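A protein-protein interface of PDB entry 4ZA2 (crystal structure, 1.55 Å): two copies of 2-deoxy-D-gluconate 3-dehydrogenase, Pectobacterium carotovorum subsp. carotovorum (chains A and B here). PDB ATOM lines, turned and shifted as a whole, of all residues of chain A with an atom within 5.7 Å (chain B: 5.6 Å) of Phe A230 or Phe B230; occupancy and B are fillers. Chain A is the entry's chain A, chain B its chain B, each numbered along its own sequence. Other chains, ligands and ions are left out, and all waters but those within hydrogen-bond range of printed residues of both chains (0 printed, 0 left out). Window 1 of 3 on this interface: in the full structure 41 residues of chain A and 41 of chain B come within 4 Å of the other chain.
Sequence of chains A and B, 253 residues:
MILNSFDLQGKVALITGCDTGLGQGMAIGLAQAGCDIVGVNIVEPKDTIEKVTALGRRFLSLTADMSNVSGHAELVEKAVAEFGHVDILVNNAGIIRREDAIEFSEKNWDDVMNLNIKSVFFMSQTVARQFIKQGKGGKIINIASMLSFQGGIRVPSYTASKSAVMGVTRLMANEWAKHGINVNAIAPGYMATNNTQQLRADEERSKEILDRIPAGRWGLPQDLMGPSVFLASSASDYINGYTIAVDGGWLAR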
ATOM      1  N   PHE A   6      10.068 -19.617   6.325  1.00  0.00           N
ATOM      2  CA  PHE A   6       8.783 -18.917   6.301  1.00  0.00           C
ATOM      3  C   PHE A   6       8.822 -17.649   5.455  1.00  0.00           C
ATOM      4  O   PHE A   6       7.779 -17.078   5.157  1.00  0.00           O
ATOM      5  CB  PHE A   6       8.339 -18.523   7.709  1.00  0.00           C
ATOM      6  CG  PHE A   6       8.121 -19.686   8.634  1.00  0.00           C
ATOM      7  CD1 PHE A   6       6.989 -20.466   8.545  1.00  0.00           C
ATOM      8  CD2 PHE A   6       9.040 -19.973   9.619  1.00  0.00           C
ATOM      9  CE1 PHE A   6       6.789 -21.525   9.416  1.00  0.00           C
ATOM     10  CE2 PHE A   6       8.850 -21.039  10.477  1.00  0.00           C
ATOM     11  CZ  PHE A   6       7.727 -21.816  10.379  1.00  0.00           C
ATOM     12  N   MET A 225      -3.453 -15.168   8.579  1.00  0.00           N
ATOM     13  CA  MET A 225      -2.181 -14.683   8.038  1.00  0.00           C
ATOM     14  C   MET A 225      -1.058 -15.707   8.233  1.00  0.00           C
ATOM     15  O   MET A 225      -0.356 -16.080   7.303  1.00  0.00           O
ATOM     16  CB  MET A 225      -1.809 -13.365   8.703  1.00  0.00           C
ATOM     17  CG  MET A 225      -2.801 -12.274   8.365  1.00  0.00           C
ATOM     18  SD  MET A 225      -2.203 -10.695   8.995  1.00  0.00           S
ATOM     19  CE  MET A 225      -3.375  -9.567   8.266  1.00  0.00           C
ATOM     20  N   GLY A 226      -0.919 -16.155   9.468  1.00  0.00           N
ATOM     21  CA  GLY A 226       0.082 -17.159   9.784  1.00  0.00           C
ATOM     22  C   GLY A 226      -0.124 -18.469   9.054  1.00  0.00           C
ATOM     23  O   GLY A 226       0.793 -18.991   8.428  1.00  0.00           O
ATOM     24  N   PRO A 227      -1.346 -19.021   9.097  1.00  0.00           N
ATOM     25  CA  PRO A 227      -1.556 -20.300   8.404  1.00  0.00           C
ATOM     26  C   PRO A 227      -1.370 -20.202   6.890  1.00  0.00           C
ATOM     27  O   PRO A 227      -0.848 -21.128   6.280  1.00  0.00           O
ATOM     28  CB  PRO A 227      -2.991 -20.677   8.792  1.00  0.00           C
ATOM     29  CG  PRO A 227      -3.161 -20.026  10.152  1.00  0.00           C
ATOM     30  CD  PRO A 227      -2.454 -18.709  10.027  1.00  0.00           C
ATOM     31  N   SER A 228      -1.782 -19.099   6.277  1.00  0.00           N
ATOM     32  CA  SER A 228      -1.589 -18.950   4.841  1.00  0.00           C
ATOM     33  C   SER A 228      -0.109 -18.784   4.472  1.00  0.00           C
ATOM     34  O   SER A 228       0.354 -19.411   3.516  1.00  0.00           O
ATOM     35  CB  SER A 228      -2.466 -17.828   4.240  1.00  0.00           C
ATOM     36  OG  SER A 228      -2.098 -16.546   4.670  1.00  0.00           O
ATOM     37  N   VAL A 229       0.641 -17.979   5.229  1.00  0.00           N
ATOM     38  CA  VAL A 229       2.100 -17.864   4.993  1.00  0.00           C
ATOM     39  C   VAL A 229       2.775 -19.235   5.121  1.00  0.00           C
ATOM     40  O   VAL A 229       3.604 -19.610   4.306  1.00  0.00           O
ATOM     41  CB  VAL A 229       2.740 -16.819   5.927  1.00  0.00           C
ATOM     42  CG1 VAL A 229       4.264 -16.888   5.868  1.00  0.00           C
ATOM     43  CG2 VAL A 229       2.244 -15.416   5.553  1.00  0.00           C
ATOM     44  N   PHE A 230       2.437 -19.960   6.177  1.00  0.00           N
ATOM     45  CA  PHE A 230       2.936 -21.303   6.423  1.00  0.00           C
ATOM     46  C   PHE A 230       2.740 -22.205   5.218  1.00  0.00           C
ATOM     47  O   PHE A 230       3.690 -22.812   4.714  1.00  0.00           O
ATOM     48  CB  PHE A 230       2.247 -21.876   7.665  1.00  0.00           C
ATOM     49  CG  PHE A 230       2.554 -23.329   7.944  1.00  0.00           C
ATOM     50  CD1 PHE A 230       3.855 -23.759   8.209  1.00  0.00           C
ATOM     51  CD2 PHE A 230       1.543 -24.266   7.961  1.00  0.00           C
ATOM     52  CE1 PHE A 230       4.106 -25.085   8.503  1.00  0.00           C
ATOM     53  CE2 PHE A 230       1.787 -25.605   8.272  1.00  0.00           C
ATOM     54  CZ  PHE A 230       3.069 -26.012   8.522  1.00  0.00           C
ATOM     55  N   LEU A 231       1.494 -22.291   4.763  1.00  0.00           N
ATOM     56  CA  LEU A 231       1.140 -23.154   3.633  1.00  0.00           C
ATOM     57  C   LEU A 231       1.694 -22.667   2.298  1.00  0.00           C
ATOM     58  O   LEU A 231       1.830 -23.454   1.371  1.00  0.00           O
ATOM     59  CB  LEU A 231      -0.381 -23.369   3.564  1.00  0.00           C
ATOM     60  CG  LEU A 231      -0.974 -24.278   4.645  1.00  0.00           C
ATOM     61  CD1 LEU A 231      -2.494 -24.326   4.507  1.00  0.00           C
ATOM     62  CD2 LEU A 231      -0.392 -25.689   4.597  1.00  0.00           C
ATOM     63  N   ALA A 232       2.034 -21.379   2.216  1.00  0.00           N
ATOM     64  CA  ALA A 232       2.611 -20.794   1.006  1.00  0.00           C
ATOM     65  C   ALA A 232       4.153 -20.877   0.994  1.00  0.00           C
ATOM     66  O   ALA A 232       4.786 -20.429   0.035  1.00  0.00           O
ATOM     67  CB  ALA A 232       2.155 -19.354   0.877  1.00  0.00           C
ATOM     68  N   SER A 233       4.749 -21.425   2.061  1.00  0.00           N
ATOM     69  CA  SER A 233       6.198 -21.394   2.277  1.00  0.00           C
ATOM     70  C   SER A 233       6.855 -22.770   2.261  1.00  0.00           C
ATOM     71  O   SER A 233       6.199 -23.801   2.330  1.00  0.00           O
ATOM     72  CB  SER A 233       6.513 -20.727   3.610  1.00  0.00           C
ATOM     73  OG  SER A 233       6.281 -21.617   4.700  1.00  0.00           O
ATOM     74  N   SER A 234       8.186 -22.771   2.180  1.00  0.00           N
ATOM     75  CA  SER A 234       8.939 -24.021   2.238  1.00  0.00           C
ATOM     76  C   SER A 234       8.837 -24.716   3.596  1.00  0.00           C
ATOM     77  O   SER A 234       9.127 -25.899   3.688  1.00  0.00           O
ATOM     78  CB  SER A 234      10.413 -23.788   1.875  1.00  0.00           C
ATOM     79  OG  SER A 234      11.032 -22.958   2.818  1.00  0.00           O
ATOM     80  N   ALA A 235       8.390 -23.999   4.626  1.00  0.00           N
ATOM     81  CA  ALA A 235       8.175 -24.609   5.952  1.00  0.00           C
ATOM     82  C   ALA A 235       7.124 -25.723   5.980  1.00  0.00           C
ATOM     83  O   ALA A 235       7.015 -26.459   6.969  1.00  0.00           O
ATOM     84  CB  ALA A 235       7.808 -23.522   6.951  1.00  0.00           C
ATOM     85  N   SER A 236       6.320 -25.836   4.921  1.00  0.00           N
ATOM     86  CA  SER A 236       5.267 -26.838   4.839  1.00  0.00           C
ATOM     87  C   SER A 236       5.416 -27.781   3.639  1.00  0.00           C
ATOM     88  O   SER A 236       4.438 -28.349   3.152  1.00  0.00           O
ATOM     89  CB  SER A 236       3.904 -26.150   4.809  1.00  0.00           C
ATOM     90  OG  SER A 236       3.762 -25.325   3.674  1.00  0.00           O
ATOM     91  N   ILE A 239       3.697 -31.172   3.560  1.00  0.00           N
ATOM     92  CA  ILE A 239       2.249 -31.169   3.742  1.00  0.00           C
ATOM     93  C   ILE A 239       1.623 -31.049   2.367  1.00  0.00           C
ATOM     94  O   ILE A 239       1.946 -30.131   1.603  1.00  0.00           O
ATOM     95  CB  ILE A 239       1.787 -30.004   4.617  1.00  0.00           C
ATOM     96  CG1 ILE A 239       2.477 -30.090   5.990  1.00  0.00           C
ATOM     97  CG2 ILE A 239       0.257 -30.033   4.750  1.00  0.00           C
ATOM     98  CD1 ILE A 239       2.076 -29.016   6.972  1.00  0.00           C
ATOM     99  N   ILE A 244      -6.406 -27.879   6.777  1.00  0.00           N
ATOM    100  CA  ILE A 244      -6.084 -27.454   8.136  1.00  0.00           C
ATOM    101  C   ILE A 244      -7.191 -26.528   8.620  1.00  0.00           C
ATOM    102  O   ILE A 244      -7.448 -25.481   7.998  1.00  0.00           O
ATOM    103  CB  ILE A 244      -4.723 -26.744   8.231  1.00  0.00           C
ATOM    104  CG1 ILE A 244      -3.610 -27.678   7.766  1.00  0.00           C
ATOM    105  CG2 ILE A 244      -4.463 -26.324   9.669  1.00  0.00           C
ATOM    106  CD1 ILE A 244      -2.231 -27.047   7.772  1.00  0.00           C
ATOM    107  N   PHE B   6       6.219 -16.045  13.897  1.00  0.00           N
ATOM    108  CA  PHE B   6       6.877 -17.356  13.866  1.00  0.00           C
ATOM    109  C   PHE B   6       8.139 -17.395  14.732  1.00  0.00           C
ATOM    110  O   PHE B   6       8.666 -18.473  14.986  1.00  0.00           O
ATOM    111  CB  PHE B   6       7.295 -17.730  12.453  1.00  0.00           C
ATOM    112  CG  PHE B   6       6.157 -17.863  11.484  1.00  0.00           C
ATOM    113  CD1 PHE B   6       5.471 -19.049  11.364  1.00  0.00           C
ATOM    114  CD2 PHE B   6       5.818 -16.814  10.659  1.00  0.00           C
ATOM    115  CE1 PHE B   6       4.434 -19.195  10.457  1.00  0.00           C
ATOM    116  CE2 PHE B   6       4.787 -16.952   9.738  1.00  0.00           C
ATOM    117  CZ  PHE B   6       4.093 -18.136   9.650  1.00  0.00           C
ATOM    118  N   MET B 225      10.360 -29.551  11.145  1.00  0.00           N
ATOM    119  CA  MET B 225      10.829 -28.328  11.769  1.00  0.00           C
ATOM    120  C   MET B 225       9.837 -27.182  11.574  1.00  0.00           C
ATOM    121  O   MET B 225       9.416 -26.533  12.534  1.00  0.00           O
ATOM    122  CB  MET B 225      12.214 -27.960  11.239  1.00  0.00           C
ATOM    123  CG  MET B 225      13.259 -28.949  11.699  1.00  0.00           C
ATOM    124  SD  MET B 225      14.855 -28.407  11.119  1.00  0.00           S
ATOM    125  CE  MET B 225      15.906 -29.694  11.819  1.00  0.00           C
ATOM    126  N   GLY B 226       9.461 -26.934  10.324  1.00  0.00           N
ATOM    127  CA  GLY B 226       8.512 -25.866  10.042  1.00  0.00           C
ATOM    128  C   GLY B 226       7.171 -26.052  10.723  1.00  0.00           C
ATOM    129  O   GLY B 226       6.682 -25.121  11.358  1.00  0.00           O
ATOM    130  N   PRO B 227       6.567 -27.244  10.574  1.00  0.00           N
ATOM    131  CA  PRO B 227       5.247 -27.496  11.199  1.00  0.00           C
ATOM    132  C   PRO B 227       5.285 -27.381  12.730  1.00  0.00           C
ATOM    133  O   PRO B 227       4.324 -26.865  13.344  1.00  0.00           O
ATOM    134  CB  PRO B 227       4.889 -28.904  10.706  1.00  0.00           C
ATOM    135  CG  PRO B 227       5.602 -29.012   9.385  1.00  0.00           C
ATOM    136  CD  PRO B 227       6.907 -28.308   9.605  1.00  0.00           C
ATOM    137  N   SER B 228       6.370 -27.838  13.344  1.00  0.00           N
ATOM    138  CA  SER B 228       6.469 -27.765  14.797  1.00  0.00           C
ATOM    139  C   SER B 228       6.673 -26.303  15.243  1.00  0.00           C
ATOM    140  O   SER B 228       6.031 -25.847  16.191  1.00  0.00           O
ATOM    141  CB  SER B 228       7.523 -28.749  15.367  1.00  0.00           C
ATOM    142  OG  SER B 228       8.831 -28.400  14.986  1.00  0.00           O
ATOM    143  N   VAL B 229       7.526 -25.542  14.565  1.00  0.00           N
ATOM    144  CA  VAL B 229       7.680 -24.137  14.891  1.00  0.00           C
ATOM    145  C   VAL B 229       6.339 -23.383  14.724  1.00  0.00           C
ATOM    146  O   VAL B 229       5.927 -22.617  15.595  1.00  0.00           O
ATOM    147  CB  VAL B 229       8.797 -23.478  14.062  1.00  0.00           C
ATOM    148  CG1 VAL B 229       8.745 -21.956  14.190  1.00  0.00           C
ATOM    149  CG2 VAL B 229      10.142 -24.029  14.513  1.00  0.00           C
ATOM    150  N   PHE B 230       5.654 -23.621  13.606  1.00  0.00           N
ATOM    151  CA  PHE B 230       4.349 -23.039  13.349  1.00  0.00           C
ATOM    152  C   PHE B 230       3.377 -23.283  14.510  1.00  0.00           C
ATOM    153  O   PHE B 230       2.786 -22.353  15.038  1.00  0.00           O
ATOM    154  CB  PHE B 230       3.813 -23.636  12.047  1.00  0.00           C
ATOM    155  CG  PHE B 230       2.383 -23.282  11.725  1.00  0.00           C
ATOM    156  CD1 PHE B 230       2.009 -21.968  11.508  1.00  0.00           C
ATOM    157  CD2 PHE B 230       1.436 -24.272  11.550  1.00  0.00           C
ATOM    158  CE1 PHE B 230       0.704 -21.652  11.155  1.00  0.00           C
ATOM    159  CE2 PHE B 230       0.127 -23.970  11.190  1.00  0.00           C
ATOM    160  CZ  PHE B 230      -0.227 -22.645  11.002  1.00  0.00           C
ATOM    161  N   LEU B 231       3.221 -24.542  14.903  1.00  0.00           N
ATOM    162  CA  LEU B 231       2.269 -24.916  15.956  1.00  0.00           C
ATOM    163  C   LEU B 231       2.728 -24.478  17.356  1.00  0.00           C
ATOM    164  O   LEU B 231       1.930 -24.452  18.273  1.00  0.00           O
ATOM    165  CB  LEU B 231       1.984 -26.434  15.943  1.00  0.00           C
ATOM    166  CG  LEU B 231       1.156 -26.945  14.759  1.00  0.00           C
ATOM    167  CD1 LEU B 231       1.064 -28.463  14.791  1.00  0.00           C
ATOM    168  CD2 LEU B 231      -0.230 -26.324  14.804  1.00  0.00           C
ATOM    169  N   ALA B 232       4.012 -24.155  17.507  1.00  0.00           N
ATOM    170  CA  ALA B 232       4.572 -23.613  18.756  1.00  0.00           C
ATOM    171  C   ALA B 232       4.542 -22.078  18.862  1.00  0.00           C
ATOM    172  O   ALA B 232       4.958 -21.499  19.872  1.00  0.00           O
ATOM    173  CB  ALA B 232       6.005 -24.102  18.911  1.00  0.00           C
ATOM    174  N   SER B 233       4.003 -21.414  17.836  1.00  0.00           N
ATOM    175  CA  SER B 233       4.123 -19.979  17.670  1.00  0.00           C
ATOM    176  C   SER B 233       2.777 -19.270  17.631  1.00  0.00           C
ATOM    177  O   SER B 233       1.745 -19.895  17.467  1.00  0.00           O
ATOM    178  CB  SER B 233       4.867 -19.679  16.377  1.00  0.00           C
ATOM    179  OG  SER B 233       4.004 -19.786  15.249  1.00  0.00           O
ATOM    180  N   SER B 234       2.844 -17.944  17.708  1.00  0.00           N
ATOM    181  CA  SER B 234       1.681 -17.054  17.584  1.00  0.00           C
ATOM    182  C   SER B 234       0.983 -17.182  16.236  1.00  0.00           C
ATOM    183  O   SER B 234      -0.207 -16.888  16.145  1.00  0.00           O
ATOM    184  CB  SER B 234       2.102 -15.594  17.788  1.00  0.00           C
ATOM    185  OG  SER B 234       2.561 -15.372  19.120  1.00  0.00           O
ATOM    186  N   ALA B 235       1.711 -17.640  15.224  1.00  0.00           N
ATOM    187  CA  ALA B 235       1.166 -17.782  13.863  1.00  0.00           C
ATOM    188  C   ALA B 235       0.034 -18.798  13.749  1.00  0.00           C
ATOM    189  O   ALA B 235      -0.669 -18.812  12.732  1.00  0.00           O
ATOM    190  CB  ALA B 235       2.279 -18.125  12.894  1.00  0.00           C
ATOM    191  N   SER B 236      -0.127 -19.668  14.744  1.00  0.00           N
ATOM    192  CA  SER B 236      -1.183 -20.687  14.726  1.00  0.00           C
ATOM    193  C   SER B 236      -2.179 -20.520  15.873  1.00  0.00           C
ATOM    194  O   SER B 236      -2.828 -21.481  16.246  1.00  0.00           O
ATOM    195  CB  SER B 236      -0.568 -22.085  14.782  1.00  0.00           C
ATOM    196  OG  SER B 236       0.198 -22.237  15.974  1.00  0.00           O
ATOM    197  N   ILE B 239      -5.655 -22.145  15.667  1.00  0.00           N
ATOM    198  CA  ILE B 239      -5.679 -23.568  15.415  1.00  0.00           C
ATOM    199  C   ILE B 239      -5.663 -24.240  16.770  1.00  0.00           C
ATOM    200  O   ILE B 239      -4.777 -23.966  17.587  1.00  0.00           O
ATOM    201  CB  ILE B 239      -4.475 -24.008  14.560  1.00  0.00           C
ATOM    202  CG1 ILE B 239      -4.491 -23.268  13.220  1.00  0.00           C
ATOM    203  CG2 ILE B 239      -4.455 -25.518  14.365  1.00  0.00           C
ATOM    204  CD1 ILE B 239      -3.384 -23.658  12.280  1.00  0.00           C
ATOM    205  N   ILE B 244      -2.488 -32.165  12.114  1.00  0.00           N
ATOM    206  CA  ILE B 244      -1.970 -31.808  10.798  1.00  0.00           C
ATOM    207  C   ILE B 244      -1.049 -32.924  10.316  1.00  0.00           C
ATOM    208  O   ILE B 244      -0.032 -33.225  10.965  1.00  0.00           O
ATOM    209  CB  ILE B 244      -1.187 -30.485  10.847  1.00  0.00           C
ATOM    210  CG1 ILE B 244      -2.078 -29.331  11.323  1.00  0.00           C
ATOM    211  CG2 ILE B 244      -0.638 -30.159   9.470  1.00  0.00           C
ATOM    212  CD1 ILE B 244      -1.365 -28.018  11.478  1.00  0.00           C
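O of Phe B230 is in hydrogen-bond range of OG of Ser B233.
OG of Ser B236 lies within hydrogen-bond range of O of Phe B230 (2.8 Å).
N of Ala B235 lies close to OG of Ser B233 (3.1 Å).
The side-chain hydroxyl (OG) of Ser A236 lies within hydrogen-bond range of the backbone carbonyl oxygen (O) of Phe A230 (2.7 Å).
N of Ala A235 lies close to OG of Ser A233, at 3.2 Å.
The backbone carbonyl oxygen (O) of Val A229 lies close to the side-chain hydroxyl (OG) of Ser A233, at 3.4 Å.
Of the 15 printed residues of chain B, 8 touch a printed residue of chain A.
Printed residues of chain B that touch a printed residue of chain A: Phe B6, Gly B226, Pro B227, Val B229, Phe B230, Ala B235, Ile B239 and Ile B244.
Hydrophobic or aromatic side chains of chain B within 4 Å of the printed part of chain A: Phe B6, Pro B227, Val B229, Phe B230, Ala B235, Ile B239 and Ile B244.
Ser A228 touches none of the printed residues of chain B.
Phe A230 touches just these residues of chain B: Gly B226 (3.8 Å), Pro B227 (3.8 Å) and Phe B230 (3.5 Å).
Printed residues of chain B within 4 Å of Ile A239: Ile B244.
Printed residues of chain A within 4 Å of Phe B6: Phe A6, Gly A226 and Val A229.
Of the printed residues of chain A, Phe B230 touches Gly A226, Pro A227 and Phe A230.
Ala B232 touches none of the printed residues of chain A.
The nearest residue of chain A that does not touch Phe B230 is Phe A6 (4.2 Å).
Phe B6 touches Phe A6 (CD1 to CE1, 3.4 Å).
Gly B226 touches Phe A6.
O of Gly A226 touches CZ of Phe B6, at 3.6 Å.
Gly A226 touches Phe B230 (O to CE1, 3.8 Å).
CA of Gly A226 touches O of Ala B235, at 3.5 Å.
Pro A227 touches Ala B235 (CD to O, 3.2 Å).
Val A229 touches Phe B6 (CG1 to CE2, 3.9 Å).
Phe A230 touches Phe B230 (CD2 to CE2, 3.5 Å).
Ile A244 touches Ile B239 (CG2 to CD1, 3.9 Å).
Ile B244 touches Ile A244 (CG2 to CD1, 3.9 Å).
Phe B6 touches its own counterpart, Phe A6.
Phe A6 touches Gly B226, and with the chains exchanged Gly A226 touches Phe B6.
Phe A6 touches Val B229, and with the chains exchanged Val A229 touches Phe B6.
Gly A226 touches Ala B235, and with the chains exchanged Ala A235 touches Gly B226.
Positions printed for both chains: 6, 225, 226, 227, 228, 229, 230, 231, 232, 233, 234, 235, 236, 239 and 244.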
